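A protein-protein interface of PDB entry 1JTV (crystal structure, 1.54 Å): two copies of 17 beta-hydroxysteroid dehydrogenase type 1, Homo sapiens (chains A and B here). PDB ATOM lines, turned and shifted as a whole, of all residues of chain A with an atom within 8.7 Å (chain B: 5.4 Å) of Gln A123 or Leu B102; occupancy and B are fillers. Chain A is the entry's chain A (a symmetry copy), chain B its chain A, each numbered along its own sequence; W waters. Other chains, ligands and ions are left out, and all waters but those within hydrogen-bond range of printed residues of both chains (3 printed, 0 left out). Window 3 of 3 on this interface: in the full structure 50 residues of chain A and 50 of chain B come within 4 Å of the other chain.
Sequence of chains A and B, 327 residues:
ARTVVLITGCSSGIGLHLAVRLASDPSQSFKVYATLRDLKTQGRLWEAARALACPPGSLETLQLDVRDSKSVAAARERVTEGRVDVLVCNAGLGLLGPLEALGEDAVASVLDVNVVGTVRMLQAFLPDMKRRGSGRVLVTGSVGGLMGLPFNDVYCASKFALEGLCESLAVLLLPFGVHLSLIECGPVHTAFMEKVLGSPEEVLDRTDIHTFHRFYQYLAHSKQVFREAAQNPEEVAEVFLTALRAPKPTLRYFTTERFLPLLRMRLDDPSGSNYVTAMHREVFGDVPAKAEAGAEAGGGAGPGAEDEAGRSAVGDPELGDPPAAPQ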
ATOM      1  N   SER A  69       7.514 -19.134  11.089  1.00  0.00           N
ATOM      2  CA  SER A  69       8.939 -19.070  11.370  1.00  0.00           C
ATOM      3  C   SER A  69       9.477 -20.303  12.102  1.00  0.00           C
ATOM      4  O   SER A  69      10.653 -20.633  11.903  1.00  0.00           O
ATOM      5  CB  SER A  69       9.304 -17.797  12.127  1.00  0.00           C
ATOM      6  OG  SER A  69       8.579 -17.755  13.342  1.00  0.00           O
ATOM      7  N   VAL A  72      10.137 -22.729   9.242  1.00  0.00           N
ATOM      8  CA  VAL A  72      11.340 -22.296   8.542  1.00  0.00           C
ATOM      9  C   VAL A  72      12.571 -22.765   9.320  1.00  0.00           C
ATOM     10  O   VAL A  72      13.478 -23.361   8.755  1.00  0.00           O
ATOM     11  CB  VAL A  72      11.401 -20.765   8.388  1.00  0.00           C
ATOM     12  CG1 VAL A  72      12.759 -20.260   7.915  1.00  0.00           C
ATOM     13  CG2 VAL A  72      10.303 -20.283   7.431  1.00  0.00           C
ATOM     14  N   ARG A  76      15.564 -25.571   8.343  1.00  0.00           N
ATOM     15  CA  ARG A  76      16.965 -25.178   8.340  1.00  0.00           C
ATOM     16  C   ARG A  76      17.810 -26.165   9.141  1.00  0.00           C
ATOM     17  O   ARG A  76      18.907 -26.566   8.726  1.00  0.00           O
ATOM     18  CB  ARG A  76      17.142 -23.764   8.891  1.00  0.00           C
ATOM     19  CG  ARG A  76      18.579 -23.249   8.903  1.00  0.00           C
ATOM     20  CD  ARG A  76      18.614 -21.947   9.715  1.00  0.00           C
ATOM     21  NE  ARG A  76      18.015 -22.241  11.011  1.00  0.00           N
ATOM     22  CZ  ARG A  76      17.410 -21.501  11.912  1.00  0.00           C
ATOM     23  NH1 ARG A  76      17.235 -20.201  11.729  1.00  0.00           N
ATOM     24  NH2 ARG A  76      16.961 -22.079  13.025  1.00  0.00           N
ATOM     25  N   LEU A  87      19.958 -20.570  -1.918  1.00  0.00           N
ATOM     26  CA  LEU A  87      18.597 -20.553  -1.404  1.00  0.00           C
ATOM     27  C   LEU A  87      17.696 -20.038  -2.549  1.00  0.00           C
ATOM     28  O   LEU A  87      18.051 -18.984  -3.084  1.00  0.00           O
ATOM     29  CB  LEU A  87      18.489 -19.519  -0.272  1.00  0.00           C
ATOM     30  CG  LEU A  87      17.097 -19.290   0.304  1.00  0.00           C
ATOM     31  CD1 LEU A  87      16.521 -20.569   0.893  1.00  0.00           C
ATOM     32  CD2 LEU A  87      17.143 -18.218   1.396  1.00  0.00           C
ATOM     33  N   CYS A  89      14.012 -18.790  -3.156  1.00  0.00           N
ATOM     34  CA  CYS A  89      12.735 -18.376  -2.600  1.00  0.00           C
ATOM     35  C   CYS A  89      11.743 -18.319  -3.768  1.00  0.00           C
ATOM     36  O   CYS A  89      11.745 -17.350  -4.544  1.00  0.00           O
ATOM     37  CB  CYS A  89      12.840 -16.991  -1.944  1.00  0.00           C
ATOM     38  SG  CYS A  89      13.983 -16.998  -0.529  1.00  0.00           S
ATOM     39  N   VAL A 115       5.512 -12.219   0.433  1.00  0.00           N
ATOM     40  CA  VAL A 115       6.420 -11.202   0.953  1.00  0.00           C
ATOM     41  C   VAL A 115       6.970 -11.575   2.326  1.00  0.00           C
ATOM     42  O   VAL A 115       8.169 -11.784   2.436  1.00  0.00           O
ATOM     43  CB  VAL A 115       5.771  -9.808   1.015  1.00  0.00           C
ATOM     44  CG1 VAL A 115       6.829  -8.745   1.276  1.00  0.00           C
ATOM     45  CG2 VAL A 115       5.028  -9.498  -0.287  1.00  0.00           C
ATOM     46  N   VAL A 116       6.082 -11.658   3.329  1.00  0.00           N
ATOM     47  CA  VAL A 116       6.621 -11.965   4.673  1.00  0.00           C
ATOM     48  C   VAL A 116       7.285 -13.335   4.697  1.00  0.00           C
ATOM     49  O   VAL A 116       8.346 -13.475   5.326  1.00  0.00           O
ATOM     50  CB  VAL A 116       5.538 -11.819   5.739  1.00  0.00           C
ATOM     51  CG1 VAL A 116       6.199 -11.974   7.128  1.00  0.00           C
ATOM     52  CG2 VAL A 116       4.830 -10.467   5.672  1.00  0.00           C
ATOM     53  N   GLY A 117       6.773 -14.350   3.973  1.00  0.00           N
ATOM     54  CA  GLY A 117       7.453 -15.629   3.922  1.00  0.00           C
ATOM     55  C   GLY A 117       8.853 -15.579   3.331  1.00  0.00           C
ATOM     56  O   GLY A 117       9.777 -16.195   3.853  1.00  0.00           O
ATOM     57  N   THR A 118       9.075 -14.708   2.322  1.00  0.00           N
ATOM     58  CA  THR A 118      10.419 -14.545   1.777  1.00  0.00           C
ATOM     59  C   THR A 118      11.303 -13.841   2.805  1.00  0.00           C
ATOM     60  O   THR A 118      12.475 -14.189   2.958  1.00  0.00           O
ATOM     61  CB  THR A 118      10.307 -13.745   0.467  1.00  0.00           C
ATOM     62  OG1 THR A 118       9.405 -14.506  -0.374  1.00  0.00           O
ATOM     63  CG2 THR A 118      11.645 -13.562  -0.200  1.00  0.00           C
ATOM     64  N   VAL A 119      10.704 -12.857   3.507  1.00  0.00           N
ATOM     65  CA  VAL A 119      11.515 -12.223   4.575  1.00  0.00           C
ATOM     66  C   VAL A 119      11.911 -13.267   5.607  1.00  0.00           C
ATOM     67  O   VAL A 119      13.079 -13.316   6.032  1.00  0.00           O
ATOM     68  CB  VAL A 119      10.720 -11.089   5.234  1.00  0.00           C
ATOM     69  CG1 VAL A 119      11.473 -10.593   6.471  1.00  0.00           C
ATOM     70  CG2 VAL A 119      10.539  -9.914   4.250  1.00  0.00           C
ATOM     71  N   ARG A 120      10.988 -14.131   6.023  1.00  0.00           N
ATOM     72  CA  ARG A 120      11.318 -15.155   7.020  1.00  0.00           C
ATOM     73  C   ARG A 120      12.448 -16.055   6.528  1.00  0.00           C
ATOM     74  O   ARG A 120      13.359 -16.416   7.287  1.00  0.00           O
ATOM     75  CB  ARG A 120      10.116 -16.010   7.387  1.00  0.00           C
ATOM     76  CG  ARG A 120       8.940 -15.293   8.043  1.00  0.00           C
ATOM     77  CD  ARG A 120       7.843 -16.287   8.456  1.00  0.00           C
ATOM     78  NE  ARG A 120       6.709 -15.577   9.075  1.00  0.00           N
ATOM     79  CZ  ARG A 120       5.634 -15.167   8.411  1.00  0.00           C
ATOM     80  NH1 ARG A 120       5.496 -15.400   7.100  1.00  0.00           N
ATOM     81  NH2 ARG A 120       4.671 -14.480   9.015  1.00  0.00           N
ATOM     82  N   MET A 121      12.412 -16.417   5.236  1.00  0.00           N
ATOM     83  CA  MET A 121      13.486 -17.270   4.715  1.00  0.00           C
ATOM     84  C   MET A 121      14.809 -16.536   4.764  1.00  0.00           C
ATOM     85  O   MET A 121      15.870 -17.073   5.101  1.00  0.00           O
ATOM     86  CB  MET A 121      13.210 -17.718   3.267  1.00  0.00           C
ATOM     87  CG  MET A 121      11.960 -18.578   3.111  1.00  0.00           C
ATOM     88  SD  MET A 121      12.141 -20.168   3.951  1.00  0.00           S
ATOM     89  CE  MET A 121      13.552 -20.868   3.090  1.00  0.00           C
ATOM     90  N   LEU A 122      14.819 -15.259   4.339  1.00  0.00           N
ATOM     91  CA  LEU A 122      16.041 -14.462   4.317  1.00  0.00           C
ATOM     92  C   LEU A 122      16.576 -14.227   5.729  1.00  0.00           C
ATOM     93  O   LEU A 122      17.777 -14.383   5.959  1.00  0.00           O
ATOM     94  CB  LEU A 122      15.807 -13.142   3.577  1.00  0.00           C
ATOM     95  CG  LEU A 122      15.475 -13.319   2.078  1.00  0.00           C
ATOM     96  CD1 LEU A 122      14.955 -12.002   1.484  1.00  0.00           C
ATOM     97  CD2 LEU A 122      16.701 -13.730   1.284  1.00  0.00           C
ATOM     98  N   GLN A 123      15.695 -13.990   6.699  1.00  0.00           N
ATOM     99  CA  GLN A 123      16.204 -13.799   8.066  1.00  0.00           C
ATOM    100  C   GLN A 123      16.819 -15.090   8.605  1.00  0.00           C
ATOM    101  O   GLN A 123      17.821 -14.987   9.314  1.00  0.00           O
ATOM    102  CB  GLN A 123      15.080 -13.360   8.990  1.00  0.00           C
ATOM    103  CG  GLN A 123      14.498 -12.002   8.608  1.00  0.00           C
ATOM    104  CD  GLN A 123      13.315 -11.656   9.491  1.00  0.00           C
ATOM    105  OE1 GLN A 123      12.376 -12.428   9.693  1.00  0.00           O
ATOM    106  NE2 GLN A 123      13.337 -10.443  10.081  1.00  0.00           N
ATOM    107  N   ALA A 124      16.272 -16.242   8.243  1.00  0.00           N
ATOM    108  CA  ALA A 124      16.764 -17.532   8.692  1.00  0.00           C
ATOM    109  C   ALA A 124      18.068 -17.955   8.040  1.00  0.00           C
ATOM    110  O   ALA A 124      18.958 -18.466   8.757  1.00  0.00           O
ATOM    111  CB  ALA A 124      15.716 -18.618   8.492  1.00  0.00           C
ATOM    112  N   PHE A 125      18.253 -17.687   6.743  1.00  0.00           N
ATOM    113  CA  PHE A 125      19.443 -18.146   6.046  1.00  0.00           C
ATOM    114  C   PHE A 125      20.484 -17.120   5.683  1.00  0.00           C
ATOM    115  O   PHE A 125      21.648 -17.496   5.462  1.00  0.00           O
ATOM    116  CB  PHE A 125      18.971 -18.845   4.728  1.00  0.00           C
ATOM    117  CG  PHE A 125      18.246 -20.124   5.023  1.00  0.00           C
ATOM    118  CD1 PHE A 125      18.941 -21.323   5.119  1.00  0.00           C
ATOM    119  CD2 PHE A 125      16.876 -20.145   5.205  1.00  0.00           C
ATOM    120  CE1 PHE A 125      18.297 -22.499   5.412  1.00  0.00           C
ATOM    121  CE2 PHE A 125      16.220 -21.330   5.493  1.00  0.00           C
ATOM    122  CZ  PHE A 125      16.923 -22.523   5.588  1.00  0.00           C
ATOM    123  N   LEU A 126      20.172 -15.819   5.629  1.00  0.00           N
ATOM    124  CA  LEU A 126      21.151 -14.814   5.270  1.00  0.00           C
ATOM    125  C   LEU A 126      22.320 -14.681   6.229  1.00  0.00           C
ATOM    126  O   LEU A 126      23.461 -14.575   5.766  1.00  0.00           O
ATOM    127  CB  LEU A 126      20.555 -13.411   5.048  1.00  0.00           C
ATOM    128  CG  LEU A 126      19.948 -13.111   3.679  1.00  0.00           C
ATOM    129  CD1 LEU A 126      19.386 -11.684   3.700  1.00  0.00           C
ATOM    130  CD2 LEU A 126      20.966 -13.292   2.566  1.00  0.00           C
ATOM    131  N   PRO A 127      22.089 -14.702   7.530  1.00  0.00           N
ATOM    132  CA  PRO A 127      23.197 -14.490   8.477  1.00  0.00           C
ATOM    133  C   PRO A 127      24.367 -15.422   8.288  1.00  0.00           C
ATOM    134  O   PRO A 127      25.513 -14.935   8.291  1.00  0.00           O
ATOM    135  CB  PRO A 127      22.520 -14.567   9.832  1.00  0.00           C
ATOM    136  CG  PRO A 127      21.117 -14.102   9.567  1.00  0.00           C
ATOM    137  CD  PRO A 127      20.786 -14.719   8.214  1.00  0.00           C
ATOM    138  N   ASP A 128      24.119 -16.704   8.070  1.00  0.00           N
ATOM    139  CA  ASP A 128      25.182 -17.674   7.832  1.00  0.00           C
ATOM    140  C   ASP A 128      25.923 -17.362   6.539  1.00  0.00           C
ATOM    141  O   ASP A 128      27.134 -17.572   6.427  1.00  0.00           O
ATOM    142  CB  ASP A 128      24.611 -19.086   7.845  1.00  0.00           C
ATOM    143  CG  ASP A 128      25.577 -20.200   8.134  1.00  0.00           C
ATOM    144  OD1 ASP A 128      26.226 -20.702   7.189  1.00  0.00           O
ATOM    145  OD2 ASP A 128      25.674 -20.603   9.313  1.00  0.00           O
ATOM    146  N   MET A 129      25.210 -16.906   5.489  1.00  0.00           N
ATOM    147  CA  MET A 129      25.901 -16.545   4.258  1.00  0.00           C
ATOM    148  C   MET A 129      26.784 -15.323   4.457  1.00  0.00           C
ATOM    149  O   MET A 129      27.919 -15.277   3.971  1.00  0.00           O
ATOM    150  CB  MET A 129      24.863 -16.252   3.148  1.00  0.00           C
ATOM    151  CG  MET A 129      24.101 -17.531   2.818  1.00  0.00           C
ATOM    152  SD  MET A 129      22.944 -17.182   1.451  1.00  0.00           S
ATOM    153  CE  MET A 129      22.268 -18.844   1.259  1.00  0.00           C
ATOM    154  N   LYS A 130      26.276 -14.312   5.157  1.00  0.00           N
ATOM    155  CA  LYS A 130      27.070 -13.095   5.384  1.00  0.00           C
ATOM    156  C   LYS A 130      28.322 -13.407   6.196  1.00  0.00           C
ATOM    157  O   LYS A 130      29.386 -12.847   5.892  1.00  0.00           O
ATOM    158  CB  LYS A 130      26.206 -12.036   6.079  1.00  0.00           C
ATOM    159  CG  LYS A 130      25.058 -11.525   5.215  1.00  0.00           C
ATOM    160  CD  LYS A 130      24.024 -10.772   6.052  1.00  0.00           C
ATOM    161  CE  LYS A 130      24.233  -9.277   5.974  1.00  0.00           C
ATOM    162  NZ  LYS A 130      23.347  -8.539   6.926  1.00  0.00           N
ATOM    163  N   ARG A 131      28.215 -14.312   7.166  1.00  0.00           N
ATOM    164  CA  ARG A 131      29.408 -14.610   7.989  1.00  0.00           C
ATOM    165  C   ARG A 131      30.417 -15.462   7.242  1.00  0.00           C
ATOM    166  O   ARG A 131      31.633 -15.320   7.476  1.00  0.00           O
ATOM    167  CB  ARG A 131      29.000 -15.137   9.343  1.00  0.00           C
ATOM    168  CG  ARG A 131      28.912 -16.602   9.618  1.00  0.00           C
ATOM    169  CD  ARG A 131      27.544 -17.153   9.877  1.00  0.00           C
ATOM    170  NE  ARG A 131      26.727 -16.553  10.919  1.00  0.00           N
ATOM    171  CZ  ARG A 131      25.630 -17.145  11.401  1.00  0.00           C
ATOM    172  NH1 ARG A 131      25.249 -18.331  10.936  1.00  0.00           N
ATOM    173  NH2 ARG A 131      24.940 -16.533  12.351  1.00  0.00           N
ATOM    174  N   LEU A 165      12.150  -5.367  -1.816  1.00  0.00           N
ATOM    175  CA  LEU A 165      12.854  -6.117  -0.784  1.00  0.00           C
ATOM    176  C   LEU A 165      14.218  -6.530  -1.285  1.00  0.00           C
ATOM    177  O   LEU A 165      15.259  -6.293  -0.630  1.00  0.00           O
ATOM    178  CB  LEU A 165      12.030  -7.389  -0.468  1.00  0.00           C
ATOM    179  CG  LEU A 165      12.748  -8.341   0.508  1.00  0.00           C
ATOM    180  CD1 LEU A 165      12.933  -7.720   1.867  1.00  0.00           C
ATOM    181  CD2 LEU A 165      11.935  -9.632   0.604  1.00  0.00           C
ATOM    182  N   LEU A 169      18.099  -5.121  -0.305  1.00  0.00           N
ATOM    183  CA  LEU A 169      19.120  -6.031   0.227  1.00  0.00           C
ATOM    184  C   LEU A 169      20.342  -6.077  -0.657  1.00  0.00           C
ATOM    185  O   LEU A 169      21.479  -6.082  -0.128  1.00  0.00           O
ATOM    186  CB  LEU A 169      18.509  -7.440   0.329  1.00  0.00           C
ATOM    187  CG  LEU A 169      17.588  -7.625   1.530  1.00  0.00           C
ATOM    188  CD1 LEU A 169      16.762  -8.904   1.415  1.00  0.00           C
ATOM    189  CD2 LEU A 169      18.417  -7.708   2.809  1.00  0.00           C
ATOM    190  N   LEU B  95      10.101   1.388   8.857  1.00  0.00           N
ATOM    191  CA  LEU B  95      10.802   0.312   9.545  1.00  0.00           C
ATOM    192  C   LEU B  95      12.234   0.335   9.020  1.00  0.00           C
ATOM    193  O   LEU B  95      12.472   0.190   7.808  1.00  0.00           O
ATOM    194  CB  LEU B  95      10.131  -1.035   9.359  1.00  0.00           C
ATOM    195  CG  LEU B  95      10.783  -2.207  10.101  1.00  0.00           C
ATOM    196  CD1 LEU B  95      10.869  -1.929  11.592  1.00  0.00           C
ATOM    197  CD2 LEU B  95       9.962  -3.478   9.851  1.00  0.00           C
ATOM    198  N   LEU B  96      13.174   0.592   9.947  1.00  0.00           N
ATOM    199  CA  LEU B  96      14.565   0.730   9.515  1.00  0.00           C
ATOM    200  C   LEU B  96      15.467  -0.204  10.303  1.00  0.00           C
ATOM    201  O   LEU B  96      15.299  -0.307  11.528  1.00  0.00           O
ATOM    202  CB  LEU B  96      14.947   2.199   9.723  1.00  0.00           C
ATOM    203  CG  LEU B  96      16.213   2.782   9.133  1.00  0.00           C
ATOM    204  CD1 LEU B  96      16.160   2.907   7.622  1.00  0.00           C
ATOM    205  CD2 LEU B  96      16.458   4.172   9.753  1.00  0.00           C
ATOM    206  N   GLY B  97      16.385  -0.885   9.637  1.00  0.00           N
ATOM    207  CA  GLY B  97      17.367  -1.707  10.347  1.00  0.00           C
ATOM    208  C   GLY B  97      17.797  -2.898   9.501  1.00  0.00           C
ATOM    209  O   GLY B  97      17.254  -3.139   8.419  1.00  0.00           O
ATOM    210  N   PRO B  98      18.796  -3.632   9.972  1.00  0.00           N
ATOM    211  CA  PRO B  98      19.252  -4.840   9.293  1.00  0.00           C
ATOM    212  C   PRO B  98      18.062  -5.789   9.196  1.00  0.00           C
ATOM    213  O   PRO B  98      17.351  -5.981  10.186  1.00  0.00           O
ATOM    214  CB  PRO B  98      20.314  -5.396  10.241  1.00  0.00           C
ATOM    215  CG  PRO B  98      20.755  -4.241  11.081  1.00  0.00           C
ATOM    216  CD  PRO B  98      19.510  -3.399  11.256  1.00  0.00           C
ATOM    217  N   LEU B  99      17.843  -6.402   8.039  1.00  0.00           N
ATOM    218  CA  LEU B  99      16.703  -7.315   7.918  1.00  0.00           C
ATOM    219  C   LEU B  99      16.575  -8.372   8.997  1.00  0.00           C
ATOM    220  O   LEU B  99      15.521  -8.532   9.635  1.00  0.00           O
ATOM    221  CB  LEU B  99      16.750  -7.997   6.525  1.00  0.00           C
ATOM    222  CG  LEU B  99      15.438  -8.769   6.268  1.00  0.00           C
ATOM    223  CD1 LEU B  99      14.363  -7.837   5.734  1.00  0.00           C
ATOM    224  CD2 LEU B  99      15.677  -9.958   5.352  1.00  0.00           C
ATOM    225  N   GLU B 100      17.675  -9.031   9.362  1.00  0.00           N
ATOM    226  CA  GLU B 100      17.665 -10.068  10.385  1.00  0.00           C
ATOM    227  C   GLU B 100      17.450  -9.547  11.805  1.00  0.00           C
ATOM    228  O   GLU B 100      17.167 -10.314  12.748  1.00  0.00           O
ATOM    229  CB  GLU B 100      18.952 -10.905  10.309  1.00  0.00           C
ATOM    230  CG  GLU B 100      20.191 -10.080  10.598  1.00  0.00           C
ATOM    231  CD  GLU B 100      20.813  -9.442   9.387  1.00  0.00           C
ATOM    232  OE1 GLU B 100      20.144  -9.134   8.376  1.00  0.00           O
ATOM    233  OE2 GLU B 100      22.049  -9.230   9.373  1.00  0.00           O
ATOM    234  N   ALA B 101      17.542  -8.243  12.008  1.00  0.00           N
ATOM    235  CA  ALA B 101      17.293  -7.615  13.295  1.00  0.00           C
ATOM    236  C   ALA B 101      15.853  -7.157  13.462  1.00  0.00           C
ATOM    237  O   ALA B 101      15.484  -6.643  14.526  1.00  0.00           O
ATOM    238  CB  ALA B 101      18.216  -6.418  13.499  1.00  0.00           C
ATOM    239  N   LEU B 102      15.035  -7.242  12.406  1.00  0.00           N
ATOM    240  CA  LEU B 102      13.649  -6.813  12.530  1.00  0.00           C
ATOM    241  C   LEU B 102      12.759  -7.904  13.102  1.00  0.00           C
ATOM    242  O   LEU B 102      12.814  -9.077  12.707  1.00  0.00           O
ATOM    243  CB  LEU B 102      13.083  -6.436  11.138  1.00  0.00           C
ATOM    244  CG  LEU B 102      13.953  -5.507  10.308  1.00  0.00           C
ATOM    245  CD1 LEU B 102      13.339  -5.339   8.914  1.00  0.00           C
ATOM    246  CD2 LEU B 102      14.112  -4.154  10.993  1.00  0.00           C
ATOM    247  N   GLY B 103      11.908  -7.534  14.064  1.00  0.00           N
ATOM    248  CA  GLY B 103      10.986  -8.500  14.633  1.00  0.00           C
ATOM    249  C   GLY B 103       9.960  -8.941  13.590  1.00  0.00           C
ATOM    250  O   GLY B 103       9.491  -8.145  12.771  1.00  0.00           O
ATOM    251  N   GLU B 104       9.597 -10.217  13.628  1.00  0.00           N
ATOM    252  CA  GLU B 104       8.600 -10.763  12.716  1.00  0.00           C
ATOM    253  C   GLU B 104       7.290  -9.992  12.815  1.00  0.00           C
ATOM    254  O   GLU B 104       6.669  -9.734  11.774  1.00  0.00           O
ATOM    255  CB  GLU B 104       8.398 -12.249  13.043  1.00  0.00           C
ATOM    256  CG  GLU B 104       7.320 -12.898  12.205  1.00  0.00           C
ATOM    257  CD  GLU B 104       7.262 -14.404  12.417  1.00  0.00           C
ATOM    258  OE1 GLU B 104       8.004 -14.917  13.279  1.00  0.00           O
ATOM    259  OE2 GLU B 104       6.451 -15.007  11.701  1.00  0.00           O
ATOM    260  N   ALA B 106       6.922  -6.811  13.693  1.00  0.00           N
ATOM    261  CA  ALA B 106       7.138  -5.492  13.108  1.00  0.00           C
ATOM    262  C   ALA B 106       7.055  -5.589  11.577  1.00  0.00           C
ATOM    263  O   ALA B 106       6.467  -4.692  10.959  1.00  0.00           O
ATOM    264  CB  ALA B 106       8.464  -4.870  13.511  1.00  0.00           C
ATOM    265  N   VAL B 107       7.633  -6.652  11.011  1.00  0.00           N
ATOM    266  CA  VAL B 107       7.543  -6.819   9.557  1.00  0.00           C
ATOM    267  C   VAL B 107       6.115  -6.989   9.105  1.00  0.00           C
ATOM    268  O   VAL B 107       5.596  -6.316   8.204  1.00  0.00           O
ATOM    269  CB  VAL B 107       8.358  -8.041   9.074  1.00  0.00           C
ATOM    270  CG1 VAL B 107       8.172  -8.306   7.582  1.00  0.00           C
ATOM    271  CG2 VAL B 107       9.825  -7.786   9.424  1.00  0.00           C
ATOM    272  N   VAL B 154      12.085  -3.808   4.237  1.00  0.00           N
ATOM    273  CA  VAL B 154      10.640  -4.052   4.411  1.00  0.00           C
ATOM    274  C   VAL B 154       9.838  -2.817   4.154  1.00  0.00           C
ATOM    275  O   VAL B 154       8.768  -2.880   3.511  1.00  0.00           O
ATOM    276  CB  VAL B 154      10.384  -4.694   5.781  1.00  0.00           C
ATOM    277  CG1 VAL B 154       8.883  -4.793   6.042  1.00  0.00           C
ATOM    278  CG2 VAL B 154      11.074  -6.040   5.863  1.00  0.00           C
ATOM    279  N   ARG B 206      21.407  -8.553  17.273  1.00  0.00           N
ATOM    280  CA  ARG B 206      20.732  -9.326  16.243  1.00  0.00           C
ATOM    281  C   ARG B 206      21.393  -9.297  14.877  1.00  0.00           C
ATOM    282  O   ARG B 206      20.770  -9.734  13.896  1.00  0.00           O
ATOM    283  CB  ARG B 206      19.286  -8.842  16.121  1.00  0.00           C
ATOM    284  CG  ARG B 206      18.548  -8.740  17.446  1.00  0.00           C
ATOM    285  CD  ARG B 206      17.056  -8.897  17.192  1.00  0.00           C
ATOM    286  NE  ARG B 206      16.279  -7.924  17.948  1.00  0.00           N
ATOM    287  CZ  ARG B 206      14.965  -7.780  17.776  1.00  0.00           C
ATOM    288  NH1 ARG B 206      14.299  -8.536  16.912  1.00  0.00           N
ATOM    289  NH2 ARG B 206      14.322  -6.869  18.493  1.00  0.00           N
HETATM  290  O   HOH W   1       5.597 -17.379  12.281  1.00  0.00           O
HETATM  291  O   HOH W   2       4.139 -12.893  11.493  1.00  0.00           O
HETATM  292  O   HOH W   3      20.846  -7.842   5.858  1.00  0.00           O
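Water W1 lies within hydrogen-bond range of the side-chain carboxylate of Glu B104 (2.6 Å) and the backbone NH of Ser A69 (2.9 Å).
Water W3 bridges the side-chain amino group of Lys A130 and the side-chain carboxylate of Glu B100.
Water W2 lies within hydrogen-bond range of the guanidinium group (NH2) of Arg A120 (3.0 Å) and the side-chain carboxylate (OE2) of Glu B104 (3.1 Å).
Among the printed residues, pairs that only touch across the chains: Leu A122 with Leu B99 (3.6 Å) and Pro A127 with Glu B100 (3.9 Å).
Of the 14 printed residues of chain B, 4 touch a printed residue of chain A.
Printed residues of chain B that touch a printed residue of chain A: Leu B99, Glu B100, Leu B102 and Glu B104.
Hydrophobic or aromatic side chains of chain B that line the printed part of chain A: Leu B99.
Among the printed residues, Asp or Glu carboxylates within 4 Å of a Lys or Arg side-chain nitrogen of the other chain: Arg A120 with Glu B104 and Lys A130 with Glu B100.
Printed residues of chain B within 4 Å of Ser A69: Glu B104 (2.9 Å).
Printed residues of chain B within 4 Å of Arg A120: Glu B104.
Gln A123 touches just these residues of chain B: Leu B99 and Leu B102.
Leu B95 touches none of the printed residues of chain A.
No residue of chain A comes within 4 Å of Gly B97.
Printed residues of chain A within 4 Å of Leu B99: Leu A122 and Gln A123.
Of the printed residues of chain A, Glu B100 touches Pro A127 (3.9 Å) and Lys A130 (2.9 Å).
No residue of chain A comes within 4 Å of Ala B101.
No residue of chain A comes within 4 Å of Gly B103.
Printed residues of chain A within 4 Å of Glu B104: Ser A69 and Arg A120.
The nearest residue of chain B that does not touch Gln A123 is Glu B100 (4.1 Å).
The nearest residue of chain A that does not touch Leu B102 is Val A119 (6.1 Å).
The nearest printed residue of chain B that does not touch Arg A120 is Leu B99 (6.3 Å).
The backbone carbonyl oxygen (O) of Leu B102 is in hydrogen-bond range of the side-chain amide nitrogen (NE2) of Gln A123, at 3.0 Å.
The side-chain carboxylate of Glu B104 lies within salt-bridge range of the guanidinium group of Arg A120, at 2.7 Å.
The side-chain amino group (NZ) of Lys A130 is in salt-bridge range of the side-chain carboxylate (OE2) of Glu B100, 2.9 Å away.
The side-chain carboxylate (OE1) of Glu B104 is in hydrogen-bond range of the side-chain hydroxyl (OG) of Ser A69 (2.9 Å).
O of Leu B99 is in hydrogen-bond range of NE2 of Gln A123 (2.9 Å).
The backbone carbonyl oxygen (O) of Pro A127 sits at hydrogen-bond distance from the guanidinium group (NE) of Arg A131 (3.3 Å).
No position is printed for both chains.
Of the 7 pairs that touch across the chains among the printed residues, none has its exchanged pair printed and touching as well.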
